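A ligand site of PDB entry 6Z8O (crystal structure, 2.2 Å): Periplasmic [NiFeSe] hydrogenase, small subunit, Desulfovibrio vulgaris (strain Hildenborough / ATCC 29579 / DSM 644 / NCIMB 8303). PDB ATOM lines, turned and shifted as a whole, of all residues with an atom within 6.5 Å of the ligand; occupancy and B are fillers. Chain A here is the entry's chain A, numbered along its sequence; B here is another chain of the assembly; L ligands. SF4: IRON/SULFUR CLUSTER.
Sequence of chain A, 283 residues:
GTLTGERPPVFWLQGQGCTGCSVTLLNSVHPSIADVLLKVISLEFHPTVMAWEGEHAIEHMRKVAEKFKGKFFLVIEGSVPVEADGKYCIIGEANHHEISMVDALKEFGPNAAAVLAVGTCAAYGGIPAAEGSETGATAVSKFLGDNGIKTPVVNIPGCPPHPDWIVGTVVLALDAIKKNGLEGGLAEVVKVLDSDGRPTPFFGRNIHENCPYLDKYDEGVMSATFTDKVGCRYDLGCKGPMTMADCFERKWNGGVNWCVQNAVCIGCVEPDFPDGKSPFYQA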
ATOM      1  N   GLY A 158     -30.774  -7.512  27.120  1.00  0.00           N
ATOM      2  CA  GLY A 158     -30.515  -8.352  28.267  1.00  0.00           C
ATOM      3  C   GLY A 158     -31.819  -8.989  28.681  1.00  0.00           C
ATOM      4  O   GLY A 158     -32.882  -8.472  28.350  1.00  0.00           O
ATOM      5  N   CYS A 159     -31.752 -10.124  29.358  1.00  0.00           N
ATOM      6  CA  CYS A 159     -32.919 -10.744  29.963  1.00  0.00           C
ATOM      7  C   CYS A 159     -32.494 -11.394  31.274  1.00  0.00           C
ATOM      8  O   CYS A 159     -32.354 -12.615  31.372  1.00  0.00           O
ATOM      9  CB  CYS A 159     -33.567 -11.770  29.023  1.00  0.00           C
ATOM     10  SG  CYS A 159     -35.227 -12.220  29.553  1.00  0.00           S
ATOM     11  N   PRO A 160     -32.247 -10.574  32.315  1.00  0.00           N
ATOM     12  CA  PRO A 160     -32.319  -9.113  32.316  1.00  0.00           C
ATOM     13  C   PRO A 160     -31.001  -8.486  31.907  1.00  0.00           C
ATOM     14  O   PRO A 160     -29.996  -9.195  31.843  1.00  0.00           O
ATOM     15  CB  PRO A 160     -32.642  -8.785  33.774  1.00  0.00           C
ATOM     16  CG  PRO A 160     -31.977  -9.895  34.552  1.00  0.00           C
ATOM     17  CD  PRO A 160     -31.851 -11.094  33.632  1.00  0.00           C
ATOM     18  N   TRP A 165     -25.069  -2.042  32.365  1.00  0.00           N
ATOM     19  CA  TRP A 165     -25.431  -1.718  30.995  1.00  0.00           C
ATOM     20  C   TRP A 165     -26.484  -0.614  30.939  1.00  0.00           C
ATOM     21  O   TRP A 165     -26.521   0.157  29.966  1.00  0.00           O
ATOM     22  CB  TRP A 165     -25.964  -2.959  30.260  1.00  0.00           C
ATOM     23  CG  TRP A 165     -25.023  -4.105  30.254  1.00  0.00           C
ATOM     24  CD1 TRP A 165     -23.690  -4.085  30.539  1.00  0.00           C
ATOM     25  CD2 TRP A 165     -25.346  -5.469  29.959  1.00  0.00           C
ATOM     26  NE1 TRP A 165     -23.164  -5.347  30.436  1.00  0.00           N
ATOM     27  CE2 TRP A 165     -24.162  -6.219  30.077  1.00  0.00           C
ATOM     28  CE3 TRP A 165     -26.533  -6.130  29.601  1.00  0.00           C
ATOM     29  CZ2 TRP A 165     -24.117  -7.589  29.852  1.00  0.00           C
ATOM     30  CZ3 TRP A 165     -26.484  -7.490  29.385  1.00  0.00           C
ATOM     31  CH2 TRP A 165     -25.288  -8.210  29.510  1.00  0.00           C
ATOM     32  N   ILE A 207     -18.581 -12.893  23.576  1.00  0.00           N
ATOM     33  CA  ILE A 207     -18.301 -13.723  24.748  1.00  0.00           C
ATOM     34  C   ILE A 207     -17.204 -14.734  24.417  1.00  0.00           C
ATOM     35  O   ILE A 207     -16.163 -14.788  25.077  1.00  0.00           O
ATOM     36  CB  ILE A 207     -19.573 -14.452  25.221  1.00  0.00           C
ATOM     37  CG1 ILE A 207     -20.704 -13.461  25.545  1.00  0.00           C
ATOM     38  CG2 ILE A 207     -19.245 -15.312  26.448  1.00  0.00           C
ATOM     39  CD1 ILE A 207     -20.576 -12.763  26.873  1.00  0.00           C
ATOM     40  N   THR A 243     -23.011 -14.528  20.765  1.00  0.00           N
ATOM     41  CA  THR A 243     -23.519 -13.518  21.681  1.00  0.00           C
ATOM     42  C   THR A 243     -22.523 -12.385  21.852  1.00  0.00           C
ATOM     43  O   THR A 243     -21.311 -12.611  21.943  1.00  0.00           O
ATOM     44  CB  THR A 243     -23.854 -14.118  23.061  1.00  0.00           C
ATOM     45  OG1 THR A 243     -24.857 -15.122  22.918  1.00  0.00           O
ATOM     46  CG2 THR A 243     -24.340 -13.039  24.013  1.00  0.00           C
ATOM     47  N   MET A 244     -23.045 -11.151  21.910  1.00  0.00           N
ATOM     48  CA  MET A 244     -22.240  -9.922  21.981  1.00  0.00           C
ATOM     49  C   MET A 244     -22.488  -9.242  23.319  1.00  0.00           C
ATOM     50  O   MET A 244     -23.451  -8.485  23.465  1.00  0.00           O
ATOM     51  CB  MET A 244     -22.604  -8.977  20.838  1.00  0.00           C
ATOM     52  CG  MET A 244     -22.394  -9.556  19.454  1.00  0.00           C
ATOM     53  SD  MET A 244     -20.644  -9.823  19.114  1.00  0.00           S
ATOM     54  CE  MET A 244     -20.049  -8.129  19.106  1.00  0.00           C
ATOM     55  N   ALA A 245     -21.611  -9.471  24.306  1.00  0.00           N
ATOM     56  CA  ALA A 245     -21.809  -8.837  25.600  1.00  0.00           C
ATOM     57  C   ALA A 245     -20.543  -8.949  26.444  1.00  0.00           C
ATOM     58  O   ALA A 245     -19.759  -9.894  26.283  1.00  0.00           O
ATOM     59  CB  ALA A 245     -22.993  -9.465  26.343  1.00  0.00           C
ATOM     60  N   ASP A 246     -20.353  -7.984  27.351  1.00  0.00           N
ATOM     61  CA  ASP A 246     -19.162  -7.930  28.200  1.00  0.00           C
ATOM     62  C   ASP A 246     -19.364  -8.632  29.541  1.00  0.00           C
ATOM     63  O   ASP A 246     -18.788  -8.195  30.548  1.00  0.00           O
ATOM     64  CB  ASP A 246     -18.745  -6.478  28.424  1.00  0.00           C
ATOM     65  CG  ASP A 246     -19.719  -5.700  29.306  1.00  0.00           C
ATOM     66  OD1 ASP A 246     -20.036  -6.155  30.421  1.00  0.00           O
ATOM     67  OD2 ASP A 246     -20.150  -4.606  28.894  1.00  0.00           O
ATOM     68  N   CYS A 247     -20.134  -9.716  29.600  1.00  0.00           N
ATOM     69  CA  CYS A 247     -20.362 -10.366  30.888  1.00  0.00           C
ATOM     70  C   CYS A 247     -19.104 -11.052  31.391  1.00  0.00           C
ATOM     71  O   CYS A 247     -18.900 -11.166  32.607  1.00  0.00           O
ATOM     72  CB  CYS A 247     -21.508 -11.370  30.797  1.00  0.00           C
ATOM     73  SG  CYS A 247     -23.086 -10.752  30.147  1.00  0.00           S
ATOM     74  N   PHE A 248     -18.253 -11.534  30.474  1.00  0.00           N
ATOM     75  CA  PHE A 248     -17.009 -12.175  30.875  1.00  0.00           C
ATOM     76  C   PHE A 248     -16.151 -11.246  31.732  1.00  0.00           C
ATOM     77  O   PHE A 248     -15.408 -11.705  32.596  1.00  0.00           O
ATOM     78  CB  PHE A 248     -16.222 -12.613  29.639  1.00  0.00           C
ATOM     79  CG  PHE A 248     -16.115 -11.559  28.568  1.00  0.00           C
ATOM     80  CD1 PHE A 248     -15.310 -10.456  28.745  1.00  0.00           C
ATOM     81  CD2 PHE A 248     -16.831 -11.673  27.392  1.00  0.00           C
ATOM     82  CE1 PHE A 248     -15.214  -9.478  27.763  1.00  0.00           C
ATOM     83  CE2 PHE A 248     -16.742 -10.715  26.413  1.00  0.00           C
ATOM     84  CZ  PHE A 248     -15.934  -9.613  26.599  1.00  0.00           C
ATOM     85  N   TRP A 252     -21.585 -10.852  37.298  1.00  0.00           N
ATOM     86  CA  TRP A 252     -22.942 -10.571  37.741  1.00  0.00           C
ATOM     87  C   TRP A 252     -23.024 -10.504  39.261  1.00  0.00           C
ATOM     88  O   TRP A 252     -22.258 -11.165  39.967  1.00  0.00           O
ATOM     89  CB  TRP A 252     -23.902 -11.633  37.208  1.00  0.00           C
ATOM     90  CG  TRP A 252     -24.319 -11.349  35.806  1.00  0.00           C
ATOM     91  CD1 TRP A 252     -23.609 -11.616  34.673  1.00  0.00           C
ATOM     92  CD2 TRP A 252     -25.534 -10.725  35.392  1.00  0.00           C
ATOM     93  NE1 TRP A 252     -24.322 -11.202  33.566  1.00  0.00           N
ATOM     94  CE2 TRP A 252     -25.501 -10.650  33.985  1.00  0.00           C
ATOM     95  CE3 TRP A 252     -26.650 -10.235  36.075  1.00  0.00           C
ATOM     96  CZ2 TRP A 252     -26.543 -10.092  33.254  1.00  0.00           C
ATOM     97  CZ3 TRP A 252     -27.682  -9.685  35.339  1.00  0.00           C
ATOM     98  CH2 TRP A 252     -27.623  -9.619  33.942  1.00  0.00           C
ATOM     99  N   TRP A 258     -20.905 -15.855  36.980  1.00  0.00           N
ATOM    100  CA  TRP A 258     -21.619 -15.475  35.764  1.00  0.00           C
ATOM    101  C   TRP A 258     -21.988 -16.737  35.001  1.00  0.00           C
ATOM    102  O   TRP A 258     -21.626 -17.861  35.376  1.00  0.00           O
ATOM    103  CB  TRP A 258     -20.812 -14.508  34.910  1.00  0.00           C
ATOM    104  CG  TRP A 258     -19.607 -15.111  34.338  1.00  0.00           C
ATOM    105  CD1 TRP A 258     -18.567 -15.657  35.016  1.00  0.00           C
ATOM    106  CD2 TRP A 258     -19.298 -15.224  32.958  1.00  0.00           C
ATOM    107  NE1 TRP A 258     -17.616 -16.115  34.133  1.00  0.00           N
ATOM    108  CE2 TRP A 258     -18.043 -15.859  32.854  1.00  0.00           C
ATOM    109  CE3 TRP A 258     -19.951 -14.854  31.781  1.00  0.00           C
ATOM    110  CZ2 TRP A 258     -17.435 -16.136  31.634  1.00  0.00           C
ATOM    111  CZ3 TRP A 258     -19.353 -15.122  30.566  1.00  0.00           C
ATOM    112  CH2 TRP A 258     -18.110 -15.759  30.510  1.00  0.00           C
ATOM    113  N   CYS A 259     -22.690 -16.532  33.883  1.00  0.00           N
ATOM    114  CA  CYS A 259     -23.476 -17.602  33.274  1.00  0.00           C
ATOM    115  C   CYS A 259     -22.611 -18.723  32.713  1.00  0.00           C
ATOM    116  O   CYS A 259     -22.939 -19.911  32.894  1.00  0.00           O
ATOM    117  CB  CYS A 259     -24.359 -17.006  32.181  1.00  0.00           C
ATOM    118  SG  CYS A 259     -25.442 -15.698  32.799  1.00  0.00           S
ATOM    119  N   VAL A 260     -21.502 -18.403  32.047  1.00  0.00           N
ATOM    120  CA  VAL A 260     -20.663 -19.465  31.488  1.00  0.00           C
ATOM    121  C   VAL A 260     -20.006 -20.243  32.607  1.00  0.00           C
ATOM    122  O   VAL A 260     -19.951 -21.482  32.578  1.00  0.00           O
ATOM    123  CB  VAL A 260     -19.608 -18.892  30.537  1.00  0.00           C
ATOM    124  CG1 VAL A 260     -18.567 -19.957  30.217  1.00  0.00           C
ATOM    125  CG2 VAL A 260     -20.258 -18.366  29.265  1.00  0.00           C
ATOM    126  N   VAL A 264     -24.327 -22.282  31.480  1.00  0.00           N
ATOM    127  CA  VAL A 264     -24.170 -21.960  30.071  1.00  0.00           C
ATOM    128  C   VAL A 264     -24.595 -20.514  29.831  1.00  0.00           C
ATOM    129  O   VAL A 264     -25.217 -19.867  30.676  1.00  0.00           O
ATOM    130  CB  VAL A 264     -24.980 -22.872  29.128  1.00  0.00           C
ATOM    131  CG1 VAL A 264     -24.460 -24.284  29.187  1.00  0.00           C
ATOM    132  CG2 VAL A 264     -26.472 -22.802  29.449  1.00  0.00           C
ATOM    133  N   CYS A 265     -24.232 -20.024  28.654  1.00  0.00           N
ATOM    134  CA  CYS A 265     -24.722 -18.757  28.131  1.00  0.00           C
ATOM    135  C   CYS A 265     -25.858 -19.053  27.164  1.00  0.00           C
ATOM    136  O   CYS A 265     -25.760 -19.957  26.330  1.00  0.00           O
ATOM    137  CB  CYS A 265     -23.604 -17.994  27.432  1.00  0.00           C
ATOM    138  SG  CYS A 265     -24.037 -16.323  26.908  1.00  0.00           S
ATOM    139  N   ILE A 266     -26.932 -18.280  27.282  1.00  0.00           N
ATOM    140  CA  ILE A 266     -28.090 -18.442  26.415  1.00  0.00           C
ATOM    141  C   ILE A 266     -28.248 -17.248  25.485  1.00  0.00           C
ATOM    142  O   ILE A 266     -29.269 -17.112  24.808  1.00  0.00           O
ATOM    143  CB  ILE A 266     -29.365 -18.678  27.242  1.00  0.00           C
ATOM    144  CG1 ILE A 266     -29.595 -17.527  28.217  1.00  0.00           C
ATOM    145  CG2 ILE A 266     -29.214 -19.957  28.064  1.00  0.00           C
ATOM    146  CD1 ILE A 266     -30.955 -17.559  28.880  1.00  0.00           C
ATOM    147  N   GLY A 267     -27.247 -16.365  25.450  1.00  0.00           N
ATOM    148  CA  GLY A 267     -27.254 -15.244  24.529  1.00  0.00           C
ATOM    149  C   GLY A 267     -28.425 -14.310  24.726  1.00  0.00           C
ATOM    150  O   GLY A 267     -29.010 -13.826  23.752  1.00  0.00           O
ATOM    151  N   CYS A 268     -28.785 -14.033  25.991  1.00  0.00           N
ATOM    152  CA  CYS A 268     -30.018 -13.305  26.264  1.00  0.00           C
ATOM    153  C   CYS A 268     -30.013 -11.901  25.673  1.00  0.00           C
ATOM    154  O   CYS A 268     -31.084 -11.313  25.512  1.00  0.00           O
ATOM    155  CB  CYS A 268     -30.260 -13.245  27.765  1.00  0.00           C
ATOM    156  SG  CYS A 268     -29.091 -12.223  28.676  1.00  0.00           S
ATOM    157  N   VAL A 269     -28.830 -11.364  25.342  1.00  0.00           N
ATOM    158  CA  VAL A 269     -28.736 -10.007  24.798  1.00  0.00           C
ATOM    159  C   VAL A 269     -29.034  -9.924  23.306  1.00  0.00           C
ATOM    160  O   VAL A 269     -29.022  -8.822  22.757  1.00  0.00           O
ATOM    161  CB  VAL A 269     -27.332  -9.399  25.017  1.00  0.00           C
ATOM    162  CG1 VAL A 269     -27.048  -9.241  26.490  1.00  0.00           C
ATOM    163  CG2 VAL A 269     -26.272 -10.275  24.368  1.00  0.00           C
ATOM    164  N   GLU A 270     -29.284 -11.064  22.637  1.00  0.00           N
ATOM    165  CA  GLU A 270     -29.315 -11.000  21.181  1.00  0.00           C
ATOM    166  C   GLU A 270     -30.745 -10.783  20.684  1.00  0.00           C
ATOM    167  O   GLU A 270     -31.714 -11.137  21.364  1.00  0.00           O
ATOM    168  CB  GLU A 270     -28.746 -12.284  20.590  1.00  0.00           C
ATOM    169  CG  GLU A 270     -27.237 -12.439  20.750  1.00  0.00           C
ATOM    170  CD  GLU A 270     -26.442 -11.510  19.836  1.00  0.00           C
ATOM    171  OE1 GLU A 270     -26.846 -11.318  18.676  1.00  0.00           O
ATOM    172  OE2 GLU A 270     -25.394 -10.980  20.282  1.00  0.00           O
ATOM    173  N   ARG B  62     -38.876 -16.013  33.269  1.00  0.00           N
ATOM    174  CA  ARG B  62     -39.222 -14.717  32.707  1.00  0.00           C
ATOM    175  C   ARG B  62     -40.693 -14.368  32.896  1.00  0.00           C
ATOM    176  O   ARG B  62     -41.110 -13.274  32.489  1.00  0.00           O
ATOM    177  CB  ARG B  62     -38.870 -14.652  31.227  1.00  0.00           C
ATOM    178  CG  ARG B  62     -37.443 -14.189  30.995  1.00  0.00           C
ATOM    179  CD  ARG B  62     -36.484 -15.365  31.001  1.00  0.00           C
ATOM    180  NE  ARG B  62     -35.086 -14.970  31.096  1.00  0.00           N
ATOM    181  CZ  ARG B  62     -34.089 -15.834  31.291  1.00  0.00           C
ATOM    182  NH1 ARG B  62     -34.355 -17.127  31.421  1.00  0.00           N
ATOM    183  NH2 ARG B  62     -32.840 -15.406  31.375  1.00  0.00           N
ATOM    184  N   ARG B 171     -26.559 -16.084  38.153  1.00  0.00           N
ATOM    185  CA  ARG B 171     -26.945 -14.693  38.222  1.00  0.00           C
ATOM    186  C   ARG B 171     -28.326 -14.582  38.833  1.00  0.00           C
ATOM    187  O   ARG B 171     -29.008 -15.581  39.086  1.00  0.00           O
ATOM    188  CB  ARG B 171     -26.901 -14.017  36.839  1.00  0.00           C
ATOM    189  CG  ARG B 171     -27.859 -14.559  35.765  1.00  0.00           C
ATOM    190  CD  ARG B 171     -28.030 -13.564  34.595  1.00  0.00           C
ATOM    191  NE  ARG B 171     -28.806 -14.105  33.486  1.00  0.00           N
ATOM    192  CZ  ARG B 171     -29.108 -13.450  32.362  1.00  0.00           C
ATOM    193  NH1 ARG B 171     -28.684 -12.206  32.184  1.00  0.00           N
ATOM    194  NH2 ARG B 171     -29.825 -14.027  31.411  1.00  0.00           N
ATOM    195  N   GLN B 176     -29.093 -19.279  36.294  1.00  0.00           N
ATOM    196  CA  GLN B 176     -28.660 -20.291  35.356  1.00  0.00           C
ATOM    197  C   GLN B 176     -28.421 -21.638  36.017  1.00  0.00           C
ATOM    198  O   GLN B 176     -28.214 -22.634  35.319  1.00  0.00           O
ATOM    199  CB  GLN B 176     -27.395 -19.811  34.649  1.00  0.00           C
ATOM    200  CG  GLN B 176     -27.686 -18.777  33.587  1.00  0.00           C
ATOM    201  CD  GLN B 176     -28.258 -19.402  32.332  1.00  0.00           C
ATOM    202  OE1 GLN B 176     -28.412 -20.618  32.252  1.00  0.00           O
ATOM    203  NE2 GLN B 176     -28.566 -18.573  31.347  1.00  0.00           N
HETATM  204 FE1  SF4 L   1     -27.125 -13.334  29.154  1.00  0.00          FE
HETATM  205 FE2  SF4 L   1     -25.055 -14.607  28.023  1.00  0.00          FE
HETATM  206 FE3  SF4 L   1     -25.378 -14.695  30.732  1.00  0.00          FE
HETATM  207 FE4  SF4 L   1     -24.551 -12.414  29.508  1.00  0.00          FE
HETATM  208  S1  SF4 L   1     -23.394 -14.398  29.611  1.00  0.00           S
HETATM  209  S2  SF4 L   1     -26.193 -12.579  31.117  1.00  0.00           S
HETATM  210  S3  SF4 L   1     -25.735 -12.469  27.533  1.00  0.00           S
HETATM  211  S4  SF4 L   1     -26.787 -15.604  29.155  1.00  0.00           S
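A sulfur (S3) of the ligand lies close to the backbone NH (N) of Cys 268 (3.8 Å).
The side-chain sulfur (SG) of Cys 247 is bound to an iron atom (FE4) of the ligand (2.3 Å).
N of Ile 266 lies close to S4 of the ligand.
FE1 of the ligand is bound by SG of Cys 268 (2.3 Å).
An iron atom (FE2) of the ligand is bound by the side-chain sulfur (SG) of Cys 265 (2.3 Å).
The indole nitrogen (NE1) of Trp 252 sits close to a sulfur (S2) of the ligand, at 3.4 Å.
S2 of the ligand lies close to NH1 of Arg 171 of chain B.
FE3 of the ligand is bound by SG of Cys 259, at 2.3 Å.
Merely in contact with the ligand: Val 269 (3.6 Å), Gly 267 (3.8 Å) and Thr 243 (3.8 Å).
Hydrophobic or aromatic side chains that line the ligand: Trp 252, Ile 266 and Val 269.
Of the 25 residues printed, 10 come within 4 Å of the ligand.
The side-chain sulfur of Cys 265 lies close to the backbone NH of Gly 267.
SG of Cys 268 lies close to NH2 of Arg 171 of chain B, at 3.4 Å.
SG of Cys 268 lies close to N of Cys 159, 3.5 Å away.
The backbone carbonyl oxygen (O) of Thr 243 lies within hydrogen-bond range of the backbone NH (N) of Ile 207 (3.2 Å).
The backbone carbonyl oxygen (O) of Cys 259 lies within hydrogen-bond range of the backbone NH (N) of Val 264.
The backbone carbonyl oxygen (O) of Cys 159 sits at hydrogen-bond distance from the guanidinium group (NH2) of Arg 171 of chain B.
NE of Arg 171 of chain B sits close to SG of Cys 259 (3.8 Å).
The side-chain sulfur (SG) of Cys 247 lies close to the indole nitrogen (NE1) of Trp 252 (3.7 Å).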
